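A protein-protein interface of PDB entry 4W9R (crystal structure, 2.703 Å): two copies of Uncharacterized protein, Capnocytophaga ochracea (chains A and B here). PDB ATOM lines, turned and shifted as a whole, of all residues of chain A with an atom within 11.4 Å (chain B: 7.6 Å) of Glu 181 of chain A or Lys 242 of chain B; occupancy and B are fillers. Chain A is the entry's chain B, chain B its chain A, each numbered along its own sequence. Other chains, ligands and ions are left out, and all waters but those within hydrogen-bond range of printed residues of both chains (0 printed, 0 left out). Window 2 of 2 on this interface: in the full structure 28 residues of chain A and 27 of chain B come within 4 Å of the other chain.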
ATOM      1  N   GLU A 123     -17.850  12.322 -15.621  1.00  0.00           N
ATOM      2  CA  GLU A 123     -18.926  12.685 -14.695  1.00  0.00           C
ATOM      3  C   GLU A 123     -18.641  14.001 -13.971  1.00  0.00           C
ATOM      4  O   GLU A 123     -18.318  15.004 -14.606  1.00  0.00           O
ATOM      5  CB  GLU A 123     -19.170  11.561 -13.683  1.00  0.00           C
ATOM      6  CG  GLU A 123     -19.891  10.344 -14.261  1.00  0.00           C
ATOM      7  CD  GLU A 123     -18.995   9.470 -15.120  1.00  0.00           C
ATOM      8  OE1 GLU A 123     -17.942   9.021 -14.619  1.00  0.00           O
ATOM      9  OE2 GLU A 123     -19.346   9.229 -16.295  1.00  0.00           O
ATOM     10  N   ASN A 148     -18.628  12.688 -20.568  1.00  0.00           N
ATOM     11  CA  ASN A 148     -19.920  12.624 -19.892  1.00  0.00           C
ATOM     12  C   ASN A 148     -19.955  13.477 -18.623  1.00  0.00           C
ATOM     13  O   ASN A 148     -20.178  12.961 -17.531  1.00  0.00           O
ATOM     14  CB  ASN A 148     -20.270  11.172 -19.551  1.00  0.00           C
ATOM     15  CG  ASN A 148     -21.661  11.029 -18.961  1.00  0.00           C
ATOM     16  OD1 ASN A 148     -22.626  11.595 -19.474  1.00  0.00           O
ATOM     17  ND2 ASN A 148     -21.763  10.295 -17.860  1.00  0.00           N
ATOM     18  N   PRO A 149     -19.719  14.788 -18.756  1.00  0.00           N
ATOM     19  CA  PRO A 149     -19.691  15.595 -17.535  1.00  0.00           C
ATOM     20  C   PRO A 149     -21.081  15.805 -16.954  1.00  0.00           C
ATOM     21  O   PRO A 149     -22.056  15.831 -17.705  1.00  0.00           O
ATOM     22  CB  PRO A 149     -19.100  16.920 -18.011  1.00  0.00           C
ATOM     23  CG  PRO A 149     -19.557  17.024 -19.426  1.00  0.00           C
ATOM     24  CD  PRO A 149     -19.542  15.614 -19.965  1.00  0.00           C
ATOM     25  N   VAL A 150     -21.169  15.941 -15.635  1.00  0.00           N
ATOM     26  CA  VAL A 150     -22.394  16.430 -15.026  1.00  0.00           C
ATOM     27  C   VAL A 150     -22.208  17.927 -14.864  1.00  0.00           C
ATOM     28  O   VAL A 150     -21.447  18.369 -14.005  1.00  0.00           O
ATOM     29  CB  VAL A 150     -22.662  15.772 -13.661  1.00  0.00           C
ATOM     30  CG1 VAL A 150     -23.977  16.266 -13.080  1.00  0.00           C
ATOM     31  CG2 VAL A 150     -22.654  14.254 -13.789  1.00  0.00           C
ATOM     32  N   THR A 177     -20.601  13.460 -24.751  1.00  0.00           N
ATOM     33  CA  THR A 177     -21.766  13.066 -23.969  1.00  0.00           C
ATOM     34  C   THR A 177     -22.606  12.036 -24.725  1.00  0.00           C
ATOM     35  O   THR A 177     -22.494  11.902 -25.944  1.00  0.00           O
ATOM     36  CB  THR A 177     -22.640  14.284 -23.604  1.00  0.00           C
ATOM     37  OG1 THR A 177     -23.754  13.855 -22.811  1.00  0.00           O
ATOM     38  CG2 THR A 177     -23.146  14.976 -24.859  1.00  0.00           C
ATOM     39  N   ALA A 178     -23.435  11.304 -23.988  1.00  0.00           N
ATOM     40  CA  ALA A 178     -24.291  10.273 -24.565  1.00  0.00           C
ATOM     41  C   ALA A 178     -25.677  10.361 -23.946  1.00  0.00           C
ATOM     42  O   ALA A 178     -25.803  10.652 -22.762  1.00  0.00           O
ATOM     43  CB  ALA A 178     -23.691   8.895 -24.350  1.00  0.00           C
ATOM     44  N   ASP A 179     -26.715  10.147 -24.748  1.00  0.00           N
ATOM     45  CA  ASP A 179     -28.085  10.328 -24.270  1.00  0.00           C
ATOM     46  C   ASP A 179     -28.800   9.086 -23.724  1.00  0.00           C
ATOM     47  O   ASP A 179     -29.868   9.219 -23.126  1.00  0.00           O
ATOM     48  CB  ASP A 179     -28.939  10.931 -25.391  1.00  0.00           C
ATOM     49  CG  ASP A 179     -29.089  10.003 -26.577  1.00  0.00           C
ATOM     50  OD1 ASP A 179     -28.154   9.218 -26.843  1.00  0.00           O
ATOM     51  OD2 ASP A 179     -30.143  10.056 -27.244  1.00  0.00           O
ATOM     52  N   VAL A 180     -28.239   7.890 -23.889  1.00  0.00           N
ATOM     53  CA  VAL A 180     -29.021   6.701 -23.550  1.00  0.00           C
ATOM     54  C   VAL A 180     -29.017   6.437 -22.048  1.00  0.00           C
ATOM     55  O   VAL A 180     -27.978   6.174 -21.442  1.00  0.00           O
ATOM     56  CB  VAL A 180     -28.510   5.449 -24.283  1.00  0.00           C
ATOM     57  CG1 VAL A 180     -29.227   4.210 -23.774  1.00  0.00           C
ATOM     58  CG2 VAL A 180     -28.710   5.599 -25.780  1.00  0.00           C
ATOM     59  N   GLU A 181     -30.217   6.517 -21.478  1.00  0.00           N
ATOM     60  CA  GLU A 181     -30.475   6.436 -20.041  1.00  0.00           C
ATOM     61  C   GLU A 181     -29.686   7.504 -19.288  1.00  0.00           C
ATOM     62  O   GLU A 181     -29.468   7.393 -18.083  1.00  0.00           O
ATOM     63  CB  GLU A 181     -30.118   5.044 -19.505  1.00  0.00           C
ATOM     64  CG  GLU A 181     -30.917   3.899 -20.115  1.00  0.00           C
ATOM     65  CD  GLU A 181     -32.254   3.679 -19.426  1.00  0.00           C
ATOM     66  OE1 GLU A 181     -32.576   4.436 -18.486  1.00  0.00           O
ATOM     67  OE2 GLU A 181     -32.983   2.742 -19.822  1.00  0.00           O
ATOM     68  N   ASN A 182     -29.238   8.521 -20.016  1.00  0.00           N
ATOM     69  CA  ASN A 182     -28.592   9.695 -19.441  1.00  0.00           C
ATOM     70  C   ASN A 182     -29.438  10.964 -19.338  1.00  0.00           C
ATOM     71  O   ASN A 182     -28.925  12.001 -18.921  1.00  0.00           O
ATOM     72  CB  ASN A 182     -27.316  10.006 -20.212  1.00  0.00           C
ATOM     73  CG  ASN A 182     -26.165  10.363 -19.298  1.00  0.00           C
ATOM     74  OD1 ASN A 182     -26.159  10.000 -18.120  1.00  0.00           O
ATOM     75  ND2 ASN A 182     -25.182  11.076 -19.832  1.00  0.00           N
ATOM     76  N   LYS A 183     -30.707  10.891 -19.736  1.00  0.00           N
ATOM     77  CA  LYS A 183     -31.440  12.066 -20.228  1.00  0.00           C
ATOM     78  C   LYS A 183     -31.315  13.343 -19.390  1.00  0.00           C
ATOM     79  O   LYS A 183     -31.104  14.423 -19.943  1.00  0.00           O
ATOM     80  CB  LYS A 183     -32.924  11.731 -20.378  1.00  0.00           C
ATOM     81  CG  LYS A 183     -33.725  12.848 -21.030  1.00  0.00           C
ATOM     82  CD  LYS A 183     -35.182  12.468 -21.216  1.00  0.00           C
ATOM     83  CE  LYS A 183     -35.930  13.549 -21.979  1.00  0.00           C
ATOM     84  NZ  LYS A 183     -35.802  14.878 -21.322  1.00  0.00           N
ATOM     85  N   VAL A 184     -31.435  13.227 -18.072  1.00  0.00           N
ATOM     86  CA  VAL A 184     -31.281  14.391 -17.203  1.00  0.00           C
ATOM     87  C   VAL A 184     -29.882  14.993 -17.334  1.00  0.00           C
ATOM     88  O   VAL A 184     -29.731  16.194 -17.567  1.00  0.00           O
ATOM     89  CB  VAL A 184     -31.547  14.038 -15.728  1.00  0.00           C
ATOM     90  CG1 VAL A 184     -31.105  15.176 -14.817  1.00  0.00           C
ATOM     91  CG2 VAL A 184     -33.020  13.718 -15.521  1.00  0.00           C
ATOM     92  N   VAL A 185     -28.868  14.145 -17.192  1.00  0.00           N
ATOM     93  CA  VAL A 185     -27.475  14.558 -17.323  1.00  0.00           C
ATOM     94  C   VAL A 185     -27.157  15.031 -18.739  1.00  0.00           C
ATOM     95  O   VAL A 185     -26.485  16.046 -18.932  1.00  0.00           O
ATOM     96  CB  VAL A 185     -26.519  13.405 -16.954  1.00  0.00           C
ATOM     97  CG1 VAL A 185     -25.073  13.792 -17.227  1.00  0.00           C
ATOM     98  CG2 VAL A 185     -26.708  13.010 -15.499  1.00  0.00           C
ATOM     99  N   TYR A 186     -27.652  14.289 -19.723  1.00  0.00           N
ATOM    100  CA  TYR A 186     -27.404  14.592 -21.128  1.00  0.00           C
ATOM    101  C   TYR A 186     -27.906  15.980 -21.520  1.00  0.00           C
ATOM    102  O   TYR A 186     -27.204  16.731 -22.199  1.00  0.00           O
ATOM    103  CB  TYR A 186     -28.057  13.530 -22.014  1.00  0.00           C
ATOM    104  CG  TYR A 186     -27.996  13.830 -23.494  1.00  0.00           C
ATOM    105  CD1 TYR A 186     -26.830  13.616 -24.218  1.00  0.00           C
ATOM    106  CD2 TYR A 186     -29.109  14.313 -24.171  1.00  0.00           C
ATOM    107  CE1 TYR A 186     -26.774  13.881 -25.571  1.00  0.00           C
ATOM    108  CE2 TYR A 186     -29.062  14.581 -25.524  1.00  0.00           C
ATOM    109  CZ  TYR A 186     -27.893  14.363 -26.221  1.00  0.00           C
ATOM    110  OH  TYR A 186     -27.842  14.631 -27.571  1.00  0.00           O
ATOM    111  N   ASP A 187     -29.119  16.315 -21.091  1.00  0.00           N
ATOM    112  CA  ASP A 187     -29.710  17.606 -21.423  1.00  0.00           C
ATOM    113  C   ASP A 187     -28.904  18.757 -20.834  1.00  0.00           C
ATOM    114  O   ASP A 187     -28.668  19.762 -21.504  1.00  0.00           O
ATOM    115  CB  ASP A 187     -31.157  17.679 -20.936  1.00  0.00           C
ATOM    116  CG  ASP A 187     -32.095  16.829 -21.769  1.00  0.00           C
ATOM    117  OD1 ASP A 187     -31.782  16.583 -22.954  1.00  0.00           O
ATOM    118  OD2 ASP A 187     -33.149  16.414 -21.241  1.00  0.00           O
ATOM    119  N   LYS A 188     -28.480  18.605 -19.584  1.00  0.00           N
ATOM    120  CA  LYS A 188     -27.683  19.632 -18.924  1.00  0.00           C
ATOM    121  C   LYS A 188     -26.346  19.819 -19.635  1.00  0.00           C
ATOM    122  O   LYS A 188     -25.831  20.932 -19.720  1.00  0.00           O
ATOM    123  CB  LYS A 188     -27.461  19.281 -17.450  1.00  0.00           C
ATOM    124  CG  LYS A 188     -28.728  19.339 -16.608  1.00  0.00           C
ATOM    125  CD  LYS A 188     -28.426  19.286 -15.117  1.00  0.00           C
ATOM    126  CE  LYS A 188     -27.735  17.988 -14.732  1.00  0.00           C
ATOM    127  NZ  LYS A 188     -27.447  17.932 -13.271  1.00  0.00           N
ATOM    128  N   ASP A 211     -21.158  14.622 -29.710  1.00  0.00           N
ATOM    129  CA  ASP A 211     -22.395  14.127 -29.128  1.00  0.00           C
ATOM    130  C   ASP A 211     -22.672  12.713 -29.622  1.00  0.00           C
ATOM    131  O   ASP A 211     -22.933  12.502 -30.806  1.00  0.00           O
ATOM    132  CB  ASP A 211     -23.562  15.057 -29.479  1.00  0.00           C
ATOM    133  CG  ASP A 211     -24.896  14.544 -28.972  1.00  0.00           C
ATOM    134  OD1 ASP A 211     -24.907  13.756 -28.004  1.00  0.00           O
ATOM    135  OD2 ASP A 211     -25.937  14.936 -29.538  1.00  0.00           O
ATOM    136  N   PHE A 212     -22.626  11.744 -28.712  1.00  0.00           N
ATOM    137  CA  PHE A 212     -22.912  10.368 -29.091  1.00  0.00           C
ATOM    138  C   PHE A 212     -24.391  10.104 -28.877  1.00  0.00           C
ATOM    139  O   PHE A 212     -24.859  10.018 -27.743  1.00  0.00           O
ATOM    140  CB  PHE A 212     -22.080   9.380 -28.268  1.00  0.00           C
ATOM    141  CG  PHE A 212     -20.601   9.472 -28.511  1.00  0.00           C
ATOM    142  CD1 PHE A 212     -19.817  10.348 -27.779  1.00  0.00           C
ATOM    143  CD2 PHE A 212     -19.990   8.666 -29.458  1.00  0.00           C
ATOM    144  CE1 PHE A 212     -18.453  10.426 -27.996  1.00  0.00           C
ATOM    145  CE2 PHE A 212     -18.628   8.740 -29.679  1.00  0.00           C
ATOM    146  CZ  PHE A 212     -17.858   9.621 -28.947  1.00  0.00           C
ATOM    147  N   LYS A 213     -25.121   9.946 -29.973  1.00  0.00           N
ATOM    148  CA  LYS A 213     -26.563   9.798 -29.893  1.00  0.00           C
ATOM    149  C   LYS A 213     -26.946   8.354 -30.176  1.00  0.00           C
ATOM    150  O   LYS A 213     -26.481   7.756 -31.145  1.00  0.00           O
ATOM    151  CB  LYS A 213     -27.258  10.750 -30.868  1.00  0.00           C
ATOM    152  CG  LYS A 213     -28.751  10.909 -30.621  1.00  0.00           C
ATOM    153  CD  LYS A 213     -29.332  12.037 -31.460  1.00  0.00           C
ATOM    154  CE  LYS A 213     -28.683  13.370 -31.119  1.00  0.00           C
ATOM    155  NZ  LYS A 213     -29.242  14.489 -31.927  1.00  0.00           N
ATOM    156  N   GLY A 214     -27.787   7.795 -29.313  1.00  0.00           N
ATOM    157  CA  GLY A 214     -28.168   6.401 -29.418  1.00  0.00           C
ATOM    158  C   GLY A 214     -27.079   5.502 -28.867  1.00  0.00           C
ATOM    159  O   GLY A 214     -27.059   4.299 -29.128  1.00  0.00           O
ATOM    160  N   SER A 215     -26.169   6.093 -28.100  1.00  0.00           N
ATOM    161  CA  SER A 215     -25.060   5.352 -27.516  1.00  0.00           C
ATOM    162  C   SER A 215     -25.133   5.326 -25.994  1.00  0.00           C
ATOM    163  O   SER A 215     -25.506   6.318 -25.366  1.00  0.00           O
ATOM    164  CB  SER A 215     -23.726   5.953 -27.958  1.00  0.00           C
ATOM    165  OG  SER A 215     -22.641   5.298 -27.323  1.00  0.00           O
ATOM    166  N   SER A 216     -24.777   4.188 -25.407  1.00  0.00           N
ATOM    167  CA  SER A 216     -24.680   4.082 -23.958  1.00  0.00           C
ATOM    168  C   SER A 216     -23.523   4.936 -23.455  1.00  0.00           C
ATOM    169  O   SER A 216     -22.541   5.149 -24.169  1.00  0.00           O
ATOM    170  CB  SER A 216     -24.496   2.627 -23.525  1.00  0.00           C
ATOM    171  OG  SER A 216     -25.688   1.884 -23.710  1.00  0.00           O
ATOM    172  N   VAL A 217     -23.647   5.419 -22.224  1.00  0.00           N
ATOM    173  CA  VAL A 217     -22.675   6.337 -21.643  1.00  0.00           C
ATOM    174  C   VAL A 217     -21.264   5.758 -21.580  1.00  0.00           C
ATOM    175  O   VAL A 217     -20.315   6.360 -22.082  1.00  0.00           O
ATOM    176  CB  VAL A 217     -23.097   6.757 -20.227  1.00  0.00           C
ATOM    177  CG1 VAL A 217     -21.986   7.535 -19.551  1.00  0.00           C
ATOM    178  CG2 VAL A 217     -24.372   7.577 -20.284  1.00  0.00           C
ATOM    179  N   ASN A 218     -21.135   4.589 -20.963  1.00  0.00           N
ATOM    180  CA  ASN A 218     -19.829   3.977 -20.752  1.00  0.00           C
ATOM    181  C   ASN A 218     -19.118   3.624 -22.054  1.00  0.00           C
ATOM    182  O   ASN A 218     -17.895   3.724 -22.146  1.00  0.00           O
ATOM    183  CB  ASN A 218     -19.971   2.733 -19.876  1.00  0.00           C
ATOM    184  CG  ASN A 218     -20.402   3.068 -18.462  1.00  0.00           C
ATOM    185  OD1 ASN A 218     -20.019   4.102 -17.914  1.00  0.00           O
ATOM    186  ND2 ASN A 218     -21.206   2.195 -17.865  1.00  0.00           N
ATOM    187  N   ALA A 219     -19.885   3.219 -23.060  1.00  0.00           N
ATOM    188  CA  ALA A 219     -19.321   2.910 -24.367  1.00  0.00           C
ATOM    189  C   ALA A 219     -18.867   4.185 -25.068  1.00  0.00           C
ATOM    190  O   ALA A 219     -17.893   4.181 -25.820  1.00  0.00           O
ATOM    191  CB  ALA A 219     -20.330   2.164 -25.220  1.00  0.00           C
ATOM    192  N   ALA A 220     -19.582   5.276 -24.816  1.00  0.00           N
ATOM    193  CA  ALA A 220     -19.250   6.563 -25.415  1.00  0.00           C
ATOM    194  C   ALA A 220     -17.970   7.136 -24.821  1.00  0.00           C
ATOM    195  O   ALA A 220     -17.186   7.776 -25.521  1.00  0.00           O
ATOM    196  CB  ALA A 220     -20.397   7.541 -25.239  1.00  0.00           C
ATOM    197  N   LYS B 237     -26.844  -5.746 -19.500  1.00  0.00           N
ATOM    198  CA  LYS B 237     -26.971  -4.463 -18.812  1.00  0.00           C
ATOM    199  C   LYS B 237     -28.141  -4.428 -17.838  1.00  0.00           C
ATOM    200  O   LYS B 237     -29.167  -5.068 -18.068  1.00  0.00           O
ATOM    201  CB  LYS B 237     -27.126  -3.321 -19.821  1.00  0.00           C
ATOM    202  CG  LYS B 237     -25.843  -2.909 -20.518  1.00  0.00           C
ATOM    203  CD  LYS B 237     -26.040  -1.615 -21.291  1.00  0.00           C
ATOM    204  CE  LYS B 237     -24.785  -1.220 -22.051  1.00  0.00           C
ATOM    205  NZ  LYS B 237     -24.431  -2.226 -23.091  1.00  0.00           N
ATOM    206  N   PRO B 238     -27.983  -3.679 -16.737  1.00  0.00           N
ATOM    207  CA  PRO B 238     -29.062  -3.455 -15.770  1.00  0.00           C
ATOM    208  C   PRO B 238     -30.252  -2.753 -16.412  1.00  0.00           C
ATOM    209  O   PRO B 238     -30.084  -2.049 -17.408  1.00  0.00           O
ATOM    210  CB  PRO B 238     -28.409  -2.559 -14.713  1.00  0.00           C
ATOM    211  CG  PRO B 238     -26.949  -2.830 -14.837  1.00  0.00           C
ATOM    212  CD  PRO B 238     -26.716  -3.069 -16.296  1.00  0.00           C
ATOM    213  N   ILE B 239     -31.438  -2.940 -15.845  1.00  0.00           N
ATOM    214  CA  ILE B 239     -32.628  -2.274 -16.354  1.00  0.00           C
ATOM    215  C   ILE B 239     -32.614  -0.808 -15.933  1.00  0.00           C
ATOM    216  O   ILE B 239     -32.542  -0.495 -14.745  1.00  0.00           O
ATOM    217  CB  ILE B 239     -33.917  -2.949 -15.847  1.00  0.00           C
ATOM    218  CG1 ILE B 239     -33.925  -4.431 -16.231  1.00  0.00           C
ATOM    219  CG2 ILE B 239     -35.146  -2.244 -16.399  1.00  0.00           C
ATOM    220  CD1 ILE B 239     -35.125  -5.190 -15.711  1.00  0.00           C
ATOM    221  N   GLY B 240     -32.683   0.088 -16.912  1.00  0.00           N
ATOM    222  CA  GLY B 240     -32.611   1.511 -16.643  1.00  0.00           C
ATOM    223  C   GLY B 240     -33.961   2.120 -16.321  1.00  0.00           C
ATOM    224  O   GLY B 240     -34.996   1.470 -16.467  1.00  0.00           O
ATOM    225  N   GLY B 241     -33.945   3.375 -15.882  1.00  0.00           N
ATOM    226  CA  GLY B 241     -35.165   4.088 -15.546  1.00  0.00           C
ATOM    227  C   GLY B 241     -36.071   4.278 -16.745  1.00  0.00           C
ATOM    228  O   GLY B 241     -37.287   4.115 -16.648  1.00  0.00           O
ATOM    229  N   LYS B 242     -35.474   4.628 -17.880  1.00  0.00           N
ATOM    230  CA  LYS B 242     -36.217   4.790 -19.124  1.00  0.00           C
ATOM    231  C   LYS B 242     -36.852   3.468 -19.548  1.00  0.00           C
ATOM    232  O   LYS B 242     -38.039   3.416 -19.870  1.00  0.00           O
ATOM    233  CB  LYS B 242     -35.301   5.317 -20.229  1.00  0.00           C
ATOM    234  CG  LYS B 242     -35.946   5.390 -21.605  1.00  0.00           C
ATOM    235  CD  LYS B 242     -36.941   6.535 -21.700  1.00  0.00           C
ATOM    236  CE  LYS B 242     -37.432   6.711 -23.131  1.00  0.00           C
ATOM    237  NZ  LYS B 242     -38.336   7.885 -23.277  1.00  0.00           N
ATOM    238  N   GLU B 243     -36.052   2.406 -19.537  1.00  0.00           N
ATOM    239  CA  GLU B 243     -36.526   1.071 -19.888  1.00  0.00           C
ATOM    240  C   GLU B 243     -37.642   0.625 -18.946  1.00  0.00           C
ATOM    241  O   GLU B 243     -38.591  -0.040 -19.360  1.00  0.00           O
ATOM    242  CB  GLU B 243     -35.367   0.070 -19.851  1.00  0.00           C
ATOM    243  CG  GLU B 243     -35.750  -1.365 -20.180  1.00  0.00           C
ATOM    244  CD  GLU B 243     -34.575  -2.322 -20.062  1.00  0.00           C
ATOM    245  OE1 GLU B 243     -33.439  -1.848 -19.841  1.00  0.00           O
ATOM    246  OE2 GLU B 243     -34.785  -3.547 -20.187  1.00  0.00           O
ATOM    247  N   PHE B 244     -37.524   1.007 -17.679  1.00  0.00           N
ATOM    248  CA  PHE B 244     -38.524   0.672 -16.672  1.00  0.00           C
ATOM    249  C   PHE B 244     -39.854   1.377 -16.935  1.00  0.00           C
ATOM    250  O   PHE B 244     -40.909   0.746 -16.923  1.00  0.00           O
ATOM    251  CB  PHE B 244     -38.008   1.028 -15.275  1.00  0.00           C
ATOM    252  CG  PHE B 244     -39.072   1.033 -14.218  1.00  0.00           C
ATOM    253  CD1 PHE B 244     -39.625  -0.153 -13.764  1.00  0.00           C
ATOM    254  CD2 PHE B 244     -39.514   2.226 -13.668  1.00  0.00           C
ATOM    255  CE1 PHE B 244     -40.603  -0.149 -12.787  1.00  0.00           C
ATOM    256  CE2 PHE B 244     -40.491   2.235 -12.691  1.00  0.00           C
ATOM    257  CZ  PHE B 244     -41.035   1.046 -12.250  1.00  0.00           C
ATOM    258  N   LYS B 245     -39.795   2.683 -17.177  1.00  0.00           N
ATOM    259  CA  LYS B 245     -40.997   3.480 -17.411  1.00  0.00           C
ATOM    260  C   LYS B 245     -41.659   3.139 -18.744  1.00  0.00           C
ATOM    261  O   LYS B 245     -42.837   3.426 -18.952  1.00  0.00           O
ATOM    262  CB  LYS B 245     -40.668   4.976 -17.364  1.00  0.00           C
ATOM    263  CG  LYS B 245     -40.208   5.471 -15.999  1.00  0.00           C
ATOM    264  CD  LYS B 245     -39.886   6.960 -16.020  1.00  0.00           C
ATOM    265  CE  LYS B 245     -39.383   7.432 -14.663  1.00  0.00           C
ATOM    266  NZ  LYS B 245     -38.989   8.870 -14.668  1.00  0.00           N
ATOM    267  N   THR B 246     -40.896   2.524 -19.641  1.00  0.00           N
ATOM    268  CA  THR B 246     -41.380   2.206 -20.979  1.00  0.00           C
ATOM    269  C   THR B 246     -41.825   0.754 -21.117  1.00  0.00           C
ATOM    270  O   THR B 246     -42.995   0.475 -21.372  1.00  0.00           O
ATOM    271  CB  THR B 246     -40.303   2.487 -22.041  1.00  0.00           C
ATOM    272  OG1 THR B 246     -39.931   3.871 -21.989  1.00  0.00           O
ATOM    273  CG2 THR B 246     -40.826   2.156 -23.429  1.00  0.00           C
ATOM    274  N   GLN B 247     -40.877  -0.163 -20.965  1.00  0.00           N
ATOM    275  CA  GLN B 247     -41.116  -1.579 -21.226  1.00  0.00           C
ATOM    276  C   GLN B 247     -41.808  -2.322 -20.083  1.00  0.00           C
ATOM    277  O   GLN B 247     -42.364  -3.400 -20.291  1.00  0.00           O
ATOM    278  CB  GLN B 247     -39.790  -2.272 -21.547  1.00  0.00           C
ATOM    279  CG  GLN B 247     -38.994  -1.597 -22.652  1.00  0.00           C
ATOM    280  CD  GLN B 247     -39.718  -1.615 -23.983  1.00  0.00           C
ATOM    281  OE1 GLN B 247     -39.700  -0.631 -24.724  1.00  0.00           O
ATOM    282  NE2 GLN B 247     -40.354  -2.738 -24.297  1.00  0.00           N
ATOM    283  N   MET B 248     -41.776  -1.753 -18.882  1.00  0.00           N
ATOM    284  CA  MET B 248     -42.284  -2.448 -17.699  1.00  0.00           C
ATOM    285  C   MET B 248     -43.537  -1.801 -17.119  1.00  0.00           C
ATOM    286  O   MET B 248     -44.599  -2.421 -17.066  1.00  0.00           O
ATOM    287  CB  MET B 248     -41.203  -2.531 -16.621  1.00  0.00           C
ATOM    288  CG  MET B 248     -39.941  -3.251 -17.063  1.00  0.00           C
ATOM    289  SD  MET B 248     -38.875  -3.887 -15.560  1.00  0.00           S
ATOM    290  CE  MET B 248     -40.054  -5.313 -14.949  1.00  0.00           C
ATOM    291  N   GLU B 249     -43.399  -0.560 -16.664  1.00  0.00           N
ATOM    292  CA  GLU B 249     -44.485   0.152 -15.995  1.00  0.00           C
ATOM    293  C   GLU B 249     -45.717   0.345 -16.884  1.00  0.00           C
ATOM    294  O   GLU B 249     -46.795   0.682 -16.396  1.00  0.00           O
ATOM    295  CB  GLU B 249     -43.986   1.510 -15.501  1.00  0.00           C
ATOM    296  CG  GLU B 249     -44.772   2.075 -14.332  1.00  0.00           C
ATOM    297  CD  GLU B 249     -44.266   3.434 -13.902  1.00  0.00           C
ATOM    298  OE1 GLU B 249     -43.734   4.167 -14.763  1.00  0.00           O
ATOM    299  OE2 GLU B 249     -44.396   3.768 -12.706  1.00  0.00           O
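Along chain A the printed residues that touch a printed residue of chain B span positions 181 to 216. Among the printed residues, 5 pairs touch across the chains. Among the printed residues, no Asp or Glu carboxylate lies within 4 Å of a Lys or Arg side-chain nitrogen of the other chain.
Among the printed residues, pairs that only touch across the chains: Glu 181 of chain A with Gly 240 of chain B (3.4 Å) and Ser 216 of chain A with Lys 237 of chain B (3.6 Å).
No position is printed for both chains. Of the 5 pairs that touch across the chains among the printed residues, none has its exchanged pair printed and touching as well.
Pro 149 of chain A touches none of the printed residues of chain B. Of the printed residues of chain B, Ser 216 of chain A touches Lys 237. Printed residues of chain A within 4 Å of Lys 237 of chain B: Ser 216. Gly 240 of chain B touches just one residue of chain A: Glu 181 (3.4 Å). Of chain A, only Glu 181 (3.1 Å) comes within 4 Å of Gly 241 of chain B. Of chain A, only Glu 181 comes within 4 Å of Lys 242 of chain B. Glu 243 of chain B touches one residue of chain A. No residue of chain A comes within 4 Å of Lys 245 of chain B. The nearest residue of chain B that does not touch Glu 181 of chain A is Ile 239 of chain B (5.3 Å). The nearest residue of chain A that does not touch Lys 242 of chain B is Lys 183 of chain A (5.9 Å). The nearest printed residue of chain A that does not touch Lys 237 of chain B is Ala 219 of chain A (6.4 Å).
The backbone carbonyl oxygen (O) of Lys 242 of chain B sits at hydrogen-bond distance from the side-chain hydroxyl (OG1) of Thr 246 of chain B (2.9 Å).
N of Lys 242 of chain B sits at hydrogen-bond distance from OE1 of Glu 181 of chain A, at 3.0 Å. The side-chain carboxylate of Glu 181 of chain A lies within hydrogen-bond range of the backbone NH of Gly 241 of chain B (3.1 Å). N of Glu 243 of chain B is in hydrogen-bond range of OE2 of Glu 181 of chain A.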
